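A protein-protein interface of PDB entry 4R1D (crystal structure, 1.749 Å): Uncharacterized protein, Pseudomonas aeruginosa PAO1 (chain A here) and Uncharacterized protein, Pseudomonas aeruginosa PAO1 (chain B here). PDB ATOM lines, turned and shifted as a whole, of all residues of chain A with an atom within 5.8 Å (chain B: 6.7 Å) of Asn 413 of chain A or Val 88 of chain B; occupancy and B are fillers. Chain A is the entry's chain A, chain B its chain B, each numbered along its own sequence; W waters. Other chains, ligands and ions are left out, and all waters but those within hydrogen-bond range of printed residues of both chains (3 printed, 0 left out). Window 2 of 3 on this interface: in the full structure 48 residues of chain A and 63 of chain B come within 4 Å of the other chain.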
ATOM      1  N   ARG A 216     -18.494 -31.597  30.537  1.00  0.00           N
ATOM      2  CA  ARG A 216     -18.760 -32.495  29.427  1.00  0.00           C
ATOM      3  C   ARG A 216     -17.524 -33.319  29.079  1.00  0.00           C
ATOM      4  O   ARG A 216     -17.620 -34.531  28.863  1.00  0.00           O
ATOM      5  CB  ARG A 216     -19.215 -31.704  28.199  1.00  0.00           C
ATOM      6  CG  ARG A 216     -19.749 -32.584  27.085  1.00  0.00           C
ATOM      7  CD  ARG A 216     -19.891 -31.808  25.780  1.00  0.00           C
ATOM      8  NE  ARG A 216     -20.904 -30.754  25.847  1.00  0.00           N
ATOM      9  CZ  ARG A 216     -22.214 -30.962  25.732  1.00  0.00           C
ATOM     10  NH1 ARG A 216     -22.685 -32.194  25.571  1.00  0.00           N
ATOM     11  NH2 ARG A 216     -23.058 -29.938  25.777  1.00  0.00           N
ATOM     12  N   ASP A 406     -19.404 -16.919  23.216  1.00  0.00           N
ATOM     13  CA  ASP A 406     -19.513 -18.282  22.717  1.00  0.00           C
ATOM     14  C   ASP A 406     -19.442 -19.285  23.877  1.00  0.00           C
ATOM     15  O   ASP A 406     -20.130 -20.312  23.856  1.00  0.00           O
ATOM     16  CB  ASP A 406     -18.439 -18.584  21.667  1.00  0.00           C
ATOM     17  CG  ASP A 406     -18.908 -18.283  20.250  1.00  0.00           C
ATOM     18  OD1 ASP A 406     -20.097 -17.951  20.106  1.00  0.00           O
ATOM     19  OD2 ASP A 406     -18.104 -18.406  19.289  1.00  0.00           O
ATOM     20  N   ILE A 408     -20.450 -18.737  26.941  1.00  0.00           N
ATOM     21  CA  ILE A 408     -21.752 -18.688  27.605  1.00  0.00           C
ATOM     22  C   ILE A 408     -22.785 -19.515  26.826  1.00  0.00           C
ATOM     23  O   ILE A 408     -23.583 -20.242  27.413  1.00  0.00           O
ATOM     24  CB  ILE A 408     -22.255 -17.228  27.808  1.00  0.00           C
ATOM     25  CG1 ILE A 408     -21.319 -16.457  28.744  1.00  0.00           C
ATOM     26  CG2 ILE A 408     -23.683 -17.216  28.385  1.00  0.00           C
ATOM     27  CD1 ILE A 408     -21.260 -17.025  30.161  1.00  0.00           C
ATOM     28  N   ASP A 409     -22.771 -19.419  25.501  1.00  0.00           N
ATOM     29  CA  ASP A 409     -23.732 -20.180  24.707  1.00  0.00           C
ATOM     30  C   ASP A 409     -23.482 -21.686  24.874  1.00  0.00           C
ATOM     31  O   ASP A 409     -24.425 -22.487  24.961  1.00  0.00           O
ATOM     32  CB  ASP A 409     -23.688 -19.740  23.233  1.00  0.00           C
ATOM     33  CG  ASP A 409     -24.248 -18.332  23.034  1.00  0.00           C
ATOM     34  OD1 ASP A 409     -24.865 -17.808  23.982  1.00  0.00           O
ATOM     35  OD2 ASP A 409     -24.091 -17.756  21.937  1.00  0.00           O
ATOM     36  N   SER A 410     -22.208 -22.059  24.942  1.00  0.00           N
ATOM     37  CA  SER A 410     -21.832 -23.448  25.243  1.00  0.00           C
ATOM     38  C   SER A 410     -22.386 -23.949  26.572  1.00  0.00           C
ATOM     39  O   SER A 410     -22.964 -25.030  26.625  1.00  0.00           O
ATOM     40  CB  SER A 410     -20.315 -23.622  25.235  1.00  0.00           C
ATOM     41  OG  SER A 410     -19.867 -24.064  23.970  1.00  0.00           O
ATOM     42  N   ILE A 411     -22.198 -23.193  27.650  1.00  0.00           N
ATOM     43  CA  ILE A 411     -22.735 -23.634  28.934  1.00  0.00           C
ATOM     44  C   ILE A 411     -24.263 -23.714  28.905  1.00  0.00           C
ATOM     45  O   ILE A 411     -24.830 -24.634  29.490  1.00  0.00           O
ATOM     46  CB  ILE A 411     -22.246 -22.789  30.166  1.00  0.00           C
ATOM     47  CG1 ILE A 411     -23.046 -21.492  30.308  1.00  0.00           C
ATOM     48  CG2 ILE A 411     -20.736 -22.560  30.114  1.00  0.00           C
ATOM     49  CD1 ILE A 411     -22.928 -20.850  31.680  1.00  0.00           C
ATOM     50  N   ALA A 412     -24.929 -22.777  28.227  1.00  0.00           N
ATOM     51  CA  ALA A 412     -26.390 -22.823  28.134  1.00  0.00           C
ATOM     52  C   ALA A 412     -26.816 -24.137  27.497  1.00  0.00           C
ATOM     53  O   ALA A 412     -27.790 -24.770  27.922  1.00  0.00           O
ATOM     54  CB  ALA A 412     -26.925 -21.635  27.323  1.00  0.00           C
ATOM     55  N   ASN A 413     -26.064 -24.562  26.489  1.00  0.00           N
ATOM     56  CA  ASN A 413     -26.382 -25.799  25.783  1.00  0.00           C
ATOM     57  C   ASN A 413     -26.131 -27.024  26.676  1.00  0.00           C
ATOM     58  O   ASN A 413     -26.945 -27.937  26.744  1.00  0.00           O
ATOM     59  CB  ASN A 413     -25.595 -25.879  24.467  1.00  0.00           C
ATOM     60  CG  ASN A 413     -25.923 -27.123  23.665  1.00  0.00           C
ATOM     61  OD1 ASN A 413     -27.079 -27.360  23.314  1.00  0.00           O
ATOM     62  ND2 ASN A 413     -24.900 -27.914  23.350  1.00  0.00           N
ATOM     63  N   PHE A 414     -25.011 -27.014  27.387  1.00  0.00           N
ATOM     64  CA  PHE A 414     -24.697 -28.098  28.319  1.00  0.00           C
ATOM     65  C   PHE A 414     -25.722 -28.169  29.447  1.00  0.00           C
ATOM     66  O   PHE A 414     -26.222 -29.239  29.767  1.00  0.00           O
ATOM     67  CB  PHE A 414     -23.283 -27.906  28.878  1.00  0.00           C
ATOM     68  CG  PHE A 414     -22.871 -28.949  29.892  1.00  0.00           C
ATOM     69  CD1 PHE A 414     -22.721 -30.275  29.520  1.00  0.00           C
ATOM     70  CD2 PHE A 414     -22.609 -28.590  31.205  1.00  0.00           C
ATOM     71  CE1 PHE A 414     -22.320 -31.240  30.443  1.00  0.00           C
ATOM     72  CE2 PHE A 414     -22.217 -29.546  32.141  1.00  0.00           C
ATOM     73  CZ  PHE A 414     -22.069 -30.876  31.753  1.00  0.00           C
ATOM     74  N   HIS A 415     -26.028 -27.025  30.051  1.00  0.00           N
ATOM     75  CA  HIS A 415     -27.072 -26.946  31.074  1.00  0.00           C
ATOM     76  C   HIS A 415     -28.385 -27.546  30.595  1.00  0.00           C
ATOM     77  O   HIS A 415     -29.019 -28.314  31.310  1.00  0.00           O
ATOM     78  CB  HIS A 415     -27.340 -25.497  31.458  1.00  0.00           C
ATOM     79  CG  HIS A 415     -26.289 -24.901  32.331  1.00  0.00           C
ATOM     80  ND1 HIS A 415     -26.217 -23.550  32.587  1.00  0.00           N
ATOM     81  CD2 HIS A 415     -25.275 -25.474  33.024  1.00  0.00           C
ATOM     82  CE1 HIS A 415     -25.197 -23.313  33.390  1.00  0.00           C
ATOM     83  NE2 HIS A 415     -24.608 -24.462  33.671  1.00  0.00           N
ATOM     84  N   GLY A 416     -28.804 -27.151  29.397  1.00  0.00           N
ATOM     85  CA  GLY A 416     -30.045 -27.645  28.823  1.00  0.00           C
ATOM     86  C   GLY A 416     -30.057 -29.150  28.619  1.00  0.00           C
ATOM     87  O   GLY A 416     -31.043 -29.814  28.932  1.00  0.00           O
ATOM     88  N   GLU A 417     -28.968 -29.692  28.080  1.00  0.00           N
ATOM     89  CA  GLU A 417     -28.848 -31.138  27.920  1.00  0.00           C
ATOM     90  C   GLU A 417     -28.887 -31.865  29.247  1.00  0.00           C
ATOM     91  O   GLU A 417     -29.596 -32.868  29.396  1.00  0.00           O
ATOM     92  CB  GLU A 417     -27.563 -31.497  27.188  1.00  0.00           C
ATOM     93  CG  GLU A 417     -27.588 -31.149  25.720  1.00  0.00           C
ATOM     94  CD  GLU A 417     -26.445 -31.808  24.978  1.00  0.00           C
ATOM     95  OE1 GLU A 417     -25.435 -31.137  24.744  1.00  0.00           O
ATOM     96  OE2 GLU A 417     -26.551 -33.008  24.647  1.00  0.00           O
ATOM     97  N   LEU A 418     -28.120 -31.380  30.220  1.00  0.00           N
ATOM     98  CA  LEU A 418     -28.124 -32.022  31.531  1.00  0.00           C
ATOM     99  C   LEU A 418     -29.509 -32.008  32.161  1.00  0.00           C
ATOM    100  O   LEU A 418     -29.938 -33.001  32.725  1.00  0.00           O
ATOM    101  CB  LEU A 418     -27.131 -31.358  32.487  1.00  0.00           C
ATOM    102  CG  LEU A 418     -25.684 -31.840  32.628  1.00  0.00           C
ATOM    103  CD1 LEU A 418     -25.056 -31.147  33.849  1.00  0.00           C
ATOM    104  CD2 LEU A 418     -25.570 -33.355  32.767  1.00  0.00           C
ATOM    105  N   HIS B  61     -23.185 -28.962  13.700  1.00  0.00           N
ATOM    106  CA  HIS B  61     -23.517 -27.824  14.540  1.00  0.00           C
ATOM    107  C   HIS B  61     -24.994 -27.958  14.887  1.00  0.00           C
ATOM    108  O   HIS B  61     -25.733 -28.656  14.189  1.00  0.00           O
ATOM    109  CB  HIS B  61     -23.252 -26.541  13.759  1.00  0.00           C
ATOM    110  CG  HIS B  61     -23.429 -25.284  14.549  1.00  0.00           C
ATOM    111  ND1 HIS B  61     -22.367 -24.569  15.062  1.00  0.00           N
ATOM    112  CD2 HIS B  61     -24.544 -24.588  14.877  1.00  0.00           C
ATOM    113  CE1 HIS B  61     -22.822 -23.496  15.686  1.00  0.00           C
ATOM    114  NE2 HIS B  61     -24.141 -23.484  15.587  1.00  0.00           N
ATOM    115  N   LYS B  62     -25.435 -27.324  15.971  1.00  0.00           N
ATOM    116  CA  LYS B  62     -26.835 -27.477  16.369  1.00  0.00           C
ATOM    117  C   LYS B  62     -27.773 -26.755  15.406  1.00  0.00           C
ATOM    118  O   LYS B  62     -28.949 -27.100  15.306  1.00  0.00           O
ATOM    119  CB  LYS B  62     -27.076 -26.994  17.804  1.00  0.00           C
ATOM    120  CG  LYS B  62     -26.318 -27.776  18.877  1.00  0.00           C
ATOM    121  CD  LYS B  62     -26.692 -29.251  18.913  1.00  0.00           C
ATOM    122  CE  LYS B  62     -25.963 -29.963  20.048  1.00  0.00           C
ATOM    123  NZ  LYS B  62     -26.194 -31.434  20.046  1.00  0.00           N
ATOM    124  N   SER B  63     -27.255 -25.755  14.702  1.00  0.00           N
ATOM    125  CA  SER B  63     -28.095 -24.970  13.800  1.00  0.00           C
ATOM    126  C   SER B  63     -27.448 -24.597  12.463  1.00  0.00           C
ATOM    127  O   SER B  63     -28.156 -24.327  11.493  1.00  0.00           O
ATOM    128  CB  SER B  63     -28.598 -23.705  14.501  1.00  0.00           C
ATOM    129  OG  SER B  63     -27.533 -22.813  14.788  1.00  0.00           O
ATOM    130  N   LYS B  64     -26.117 -24.586  12.404  1.00  0.00           N
ATOM    131  CA  LYS B  64     -25.411 -24.096  11.220  1.00  0.00           C
ATOM    132  C   LYS B  64     -24.900 -25.176  10.262  1.00  0.00           C
ATOM    133  O   LYS B  64     -24.136 -24.874   9.340  1.00  0.00           O
ATOM    134  CB  LYS B  64     -24.243 -23.191  11.623  1.00  0.00           C
ATOM    135  CG  LYS B  64     -24.638 -21.978  12.445  1.00  0.00           C
ATOM    136  CD  LYS B  64     -23.495 -20.978  12.495  1.00  0.00           C
ATOM    137  CE  LYS B  64     -23.836 -19.785  13.375  1.00  0.00           C
ATOM    138  NZ  LYS B  64     -24.993 -19.003  12.863  1.00  0.00           N
ATOM    139  N   MET B  67     -19.869 -29.038  10.882  1.00  0.00           N
ATOM    140  CA  MET B  67     -18.887 -28.465  11.792  1.00  0.00           C
ATOM    141  C   MET B  67     -17.606 -28.088  11.067  1.00  0.00           C
ATOM    142  O   MET B  67     -16.881 -27.199  11.507  1.00  0.00           O
ATOM    143  CB  MET B  67     -18.583 -29.419  12.960  1.00  0.00           C
ATOM    144  CG  MET B  67     -19.683 -29.469  14.007  1.00  0.00           C
ATOM    145  SD  MET B  67     -19.852 -27.910  14.871  1.00  0.00           S
ATOM    146  CE  MET B  67     -18.353 -27.911  15.872  1.00  0.00           C
ATOM    147  N   TRP B  84     -16.115 -24.869  13.411  1.00  0.00           N
ATOM    148  CA  TRP B  84     -16.752 -24.125  14.499  1.00  0.00           C
ATOM    149  C   TRP B  84     -16.127 -24.536  15.833  1.00  0.00           C
ATOM    150  O   TRP B  84     -15.773 -25.694  16.019  1.00  0.00           O
ATOM    151  CB  TRP B  84     -18.263 -24.378  14.515  1.00  0.00           C
ATOM    152  CG  TRP B  84     -18.978 -23.599  13.451  1.00  0.00           C
ATOM    153  CD1 TRP B  84     -19.655 -24.102  12.377  1.00  0.00           C
ATOM    154  CD2 TRP B  84     -19.071 -22.175  13.355  1.00  0.00           C
ATOM    155  NE1 TRP B  84     -20.168 -23.073  11.616  1.00  0.00           N
ATOM    156  CE2 TRP B  84     -19.822 -21.881  12.196  1.00  0.00           C
ATOM    157  CE3 TRP B  84     -18.591 -21.116  14.132  1.00  0.00           C
ATOM    158  CZ2 TRP B  84     -20.106 -20.577  11.806  1.00  0.00           C
ATOM    159  CZ3 TRP B  84     -18.878 -19.822  13.743  1.00  0.00           C
ATOM    160  CH2 TRP B  84     -19.628 -19.564  12.589  1.00  0.00           C
ATOM    161  N   SER B  85     -16.000 -23.596  16.767  1.00  0.00           N
ATOM    162  CA  SER B  85     -15.338 -23.899  18.038  1.00  0.00           C
ATOM    163  C   SER B  85     -16.197 -24.739  18.988  1.00  0.00           C
ATOM    164  O   SER B  85     -15.691 -25.295  19.966  1.00  0.00           O
ATOM    165  CB  SER B  85     -14.871 -22.621  18.728  1.00  0.00           C
ATOM    166  OG  SER B  85     -15.973 -21.823  19.082  1.00  0.00           O
ATOM    167  N   SER B  86     -17.496 -24.817  18.711  1.00  0.00           N
ATOM    168  CA  SER B  86     -18.393 -25.734  19.409  1.00  0.00           C
ATOM    169  C   SER B  86     -19.647 -25.918  18.582  1.00  0.00           C
ATOM    170  O   SER B  86     -19.841 -25.237  17.574  1.00  0.00           O
ATOM    171  CB  SER B  86     -18.794 -25.203  20.787  1.00  0.00           C
ATOM    172  OG  SER B  86     -19.893 -24.315  20.668  1.00  0.00           O
ATOM    173  N   GLU B  87     -20.514 -26.820  19.025  1.00  0.00           N
ATOM    174  CA  GLU B  87     -21.729 -27.088  18.275  1.00  0.00           C
ATOM    175  C   GLU B  87     -22.789 -26.001  18.415  1.00  0.00           C
ATOM    176  O   GLU B  87     -23.863 -26.105  17.818  1.00  0.00           O
ATOM    177  CB  GLU B  87     -22.277 -28.476  18.618  1.00  0.00           C
ATOM    178  CG  GLU B  87     -21.312 -29.569  18.187  1.00  0.00           C
ATOM    179  CD  GLU B  87     -21.824 -30.969  18.440  1.00  0.00           C
ATOM    180  OE1 GLU B  87     -22.906 -31.117  19.053  1.00  0.00           O
ATOM    181  OE2 GLU B  87     -21.132 -31.924  18.020  1.00  0.00           O
ATOM    182  N   VAL B  88     -22.500 -24.966  19.201  1.00  0.00           N
ATOM    183  CA  VAL B  88     -23.389 -23.801  19.254  1.00  0.00           C
ATOM    184  C   VAL B  88     -22.659 -22.480  19.042  1.00  0.00           C
ATOM    185  O   VAL B  88     -23.254 -21.406  19.174  1.00  0.00           O
ATOM    186  CB  VAL B  88     -24.198 -23.722  20.564  1.00  0.00           C
ATOM    187  CG1 VAL B  88     -25.037 -24.988  20.743  1.00  0.00           C
ATOM    188  CG2 VAL B  88     -23.274 -23.477  21.759  1.00  0.00           C
ATOM    189  N   ALA B  89     -21.380 -22.553  18.691  1.00  0.00           N
ATOM    190  CA  ALA B  89     -20.583 -21.347  18.471  1.00  0.00           C
ATOM    191  C   ALA B  89     -21.147 -20.500  17.332  1.00  0.00           C
ATOM    192  O   ALA B  89     -21.676 -21.032  16.364  1.00  0.00           O
ATOM    193  CB  ALA B  89     -19.127 -21.721  18.174  1.00  0.00           C
ATOM    194  N   SER B  90     -21.022 -19.185  17.451  1.00  0.00           N
ATOM    195  CA  SER B  90     -21.420 -18.290  16.367  1.00  0.00           C
ATOM    196  C   SER B  90     -20.381 -17.203  16.099  1.00  0.00           C
ATOM    197  O   SER B  90     -20.424 -16.532  15.061  1.00  0.00           O
ATOM    198  CB  SER B  90     -22.774 -17.653  16.674  1.00  0.00           C
ATOM    199  OG  SER B  90     -22.674 -16.770  17.768  1.00  0.00           O
ATOM    200  N   LYS B  91     -19.444 -17.020  17.027  1.00  0.00           N
ATOM    201  CA  LYS B  91     -18.480 -15.926  16.888  1.00  0.00           C
ATOM    202  C   LYS B  91     -17.028 -16.369  16.752  1.00  0.00           C
ATOM    203  O   LYS B  91     -16.155 -15.559  16.410  1.00  0.00           O
ATOM    204  CB  LYS B  91     -18.622 -14.958  18.051  1.00  0.00           C
ATOM    205  CG  LYS B  91     -20.064 -14.522  18.251  1.00  0.00           C
ATOM    206  CD  LYS B  91     -20.170 -13.364  19.219  1.00  0.00           C
ATOM    207  CE  LYS B  91     -21.609 -12.847  19.305  1.00  0.00           C
ATOM    208  NZ  LYS B  91     -22.456 -13.637  20.250  1.00  0.00           N
HETATM  209  O   HOH W   1     -21.841 -16.158  21.007  1.00  0.00           O
HETATM  210  O   HOH W   2     -23.642 -18.829  19.468  1.00  0.00           O
HETATM  211  O   HOH W   3     -19.415 -21.968  21.633  1.00  0.00           O
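Water W3 lies within hydrogen-bond range of OG of Ser 86 of chain B, O of Asp 406 of chain A and OG of Ser 410 of chain A. Water W2 lies within hydrogen-bond range of O of Val 88 of chain B, OD2 of Asp 409 of chain A and OG of Ser 90 of chain B. Water W1 lies within hydrogen-bond range of OD1 of Asp 406 of chain A (2.7 Å), NZ of Lys 91 of chain B (2.7 Å), OD2 of Asp 409 of chain A (2.9 Å) and OG of Ser 90 of chain B (3.4 Å).
N of Val 88 of chain B is in hydrogen-bond range of OG of Ser 86 of chain B. OG of Ser 86 of chain B is in hydrogen-bond range of N of Ala 89 of chain B (3.0 Å).
OD2 of Asp 406 of chain A touches CB of Ala 89 of chain B (3.6 Å). Asp 409 of chain A touches Val 88 of chain B. Val 88 of chain B touches Ser 410 of chain A (CG2 to N, 3.6 Å). Asn 413 of chain A touches Val 88 of chain B (CG to CG1, 3.7 Å).
Printed residues of chain B within 4 Å of Asp 409 of chain A: Val 88 (3.5 Å). Printed residues of chain B within 4 Å of Ser 410 of chain A: Ser 86 and Val 88. Asn 413 of chain A touches just one residue of chain B: Val 88. Of the printed residues of chain A, Ser 86 of chain B touches Ser 410 (3.3 Å). Val 88 of chain B touches three residues of chain A. Of the printed residues of chain A, Ser 90 of chain B touches Asp 406. Of the printed residues of chain A, Lys 91 of chain B touches Asp 406 (3.0 Å). The nearest residue of chain B that does not touch Asn 413 of chain A is Lys 62 of chain B (4.03 Å).
Hydrophobic or aromatic side chains of chain B within 4 Å of the printed part of chain A: Val 88 and Ala 89. Along chain B the printed residues that touch a printed residue of chain A span positions 86 to 91. Among the printed residues, 7 pairs touch across the chains. Among the printed residues, no Asp or Glu carboxylate lies within 4 Å of a Lys or Arg side-chain nitrogen of the other chain.
The side-chain carboxylate (OD1) of Asp 406 of chain A sits at hydrogen-bond distance from the backbone NH (N) of Ser 90 of chain B, at 3.1 Å. OD2 of Asp 406 of chain A is in hydrogen-bond range of N of Lys 91 of chain B, at 3.0 Å. OG of Ser 410 of chain A sits at hydrogen-bond distance from OG of Ser 86 of chain B, 3.3 Å away.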
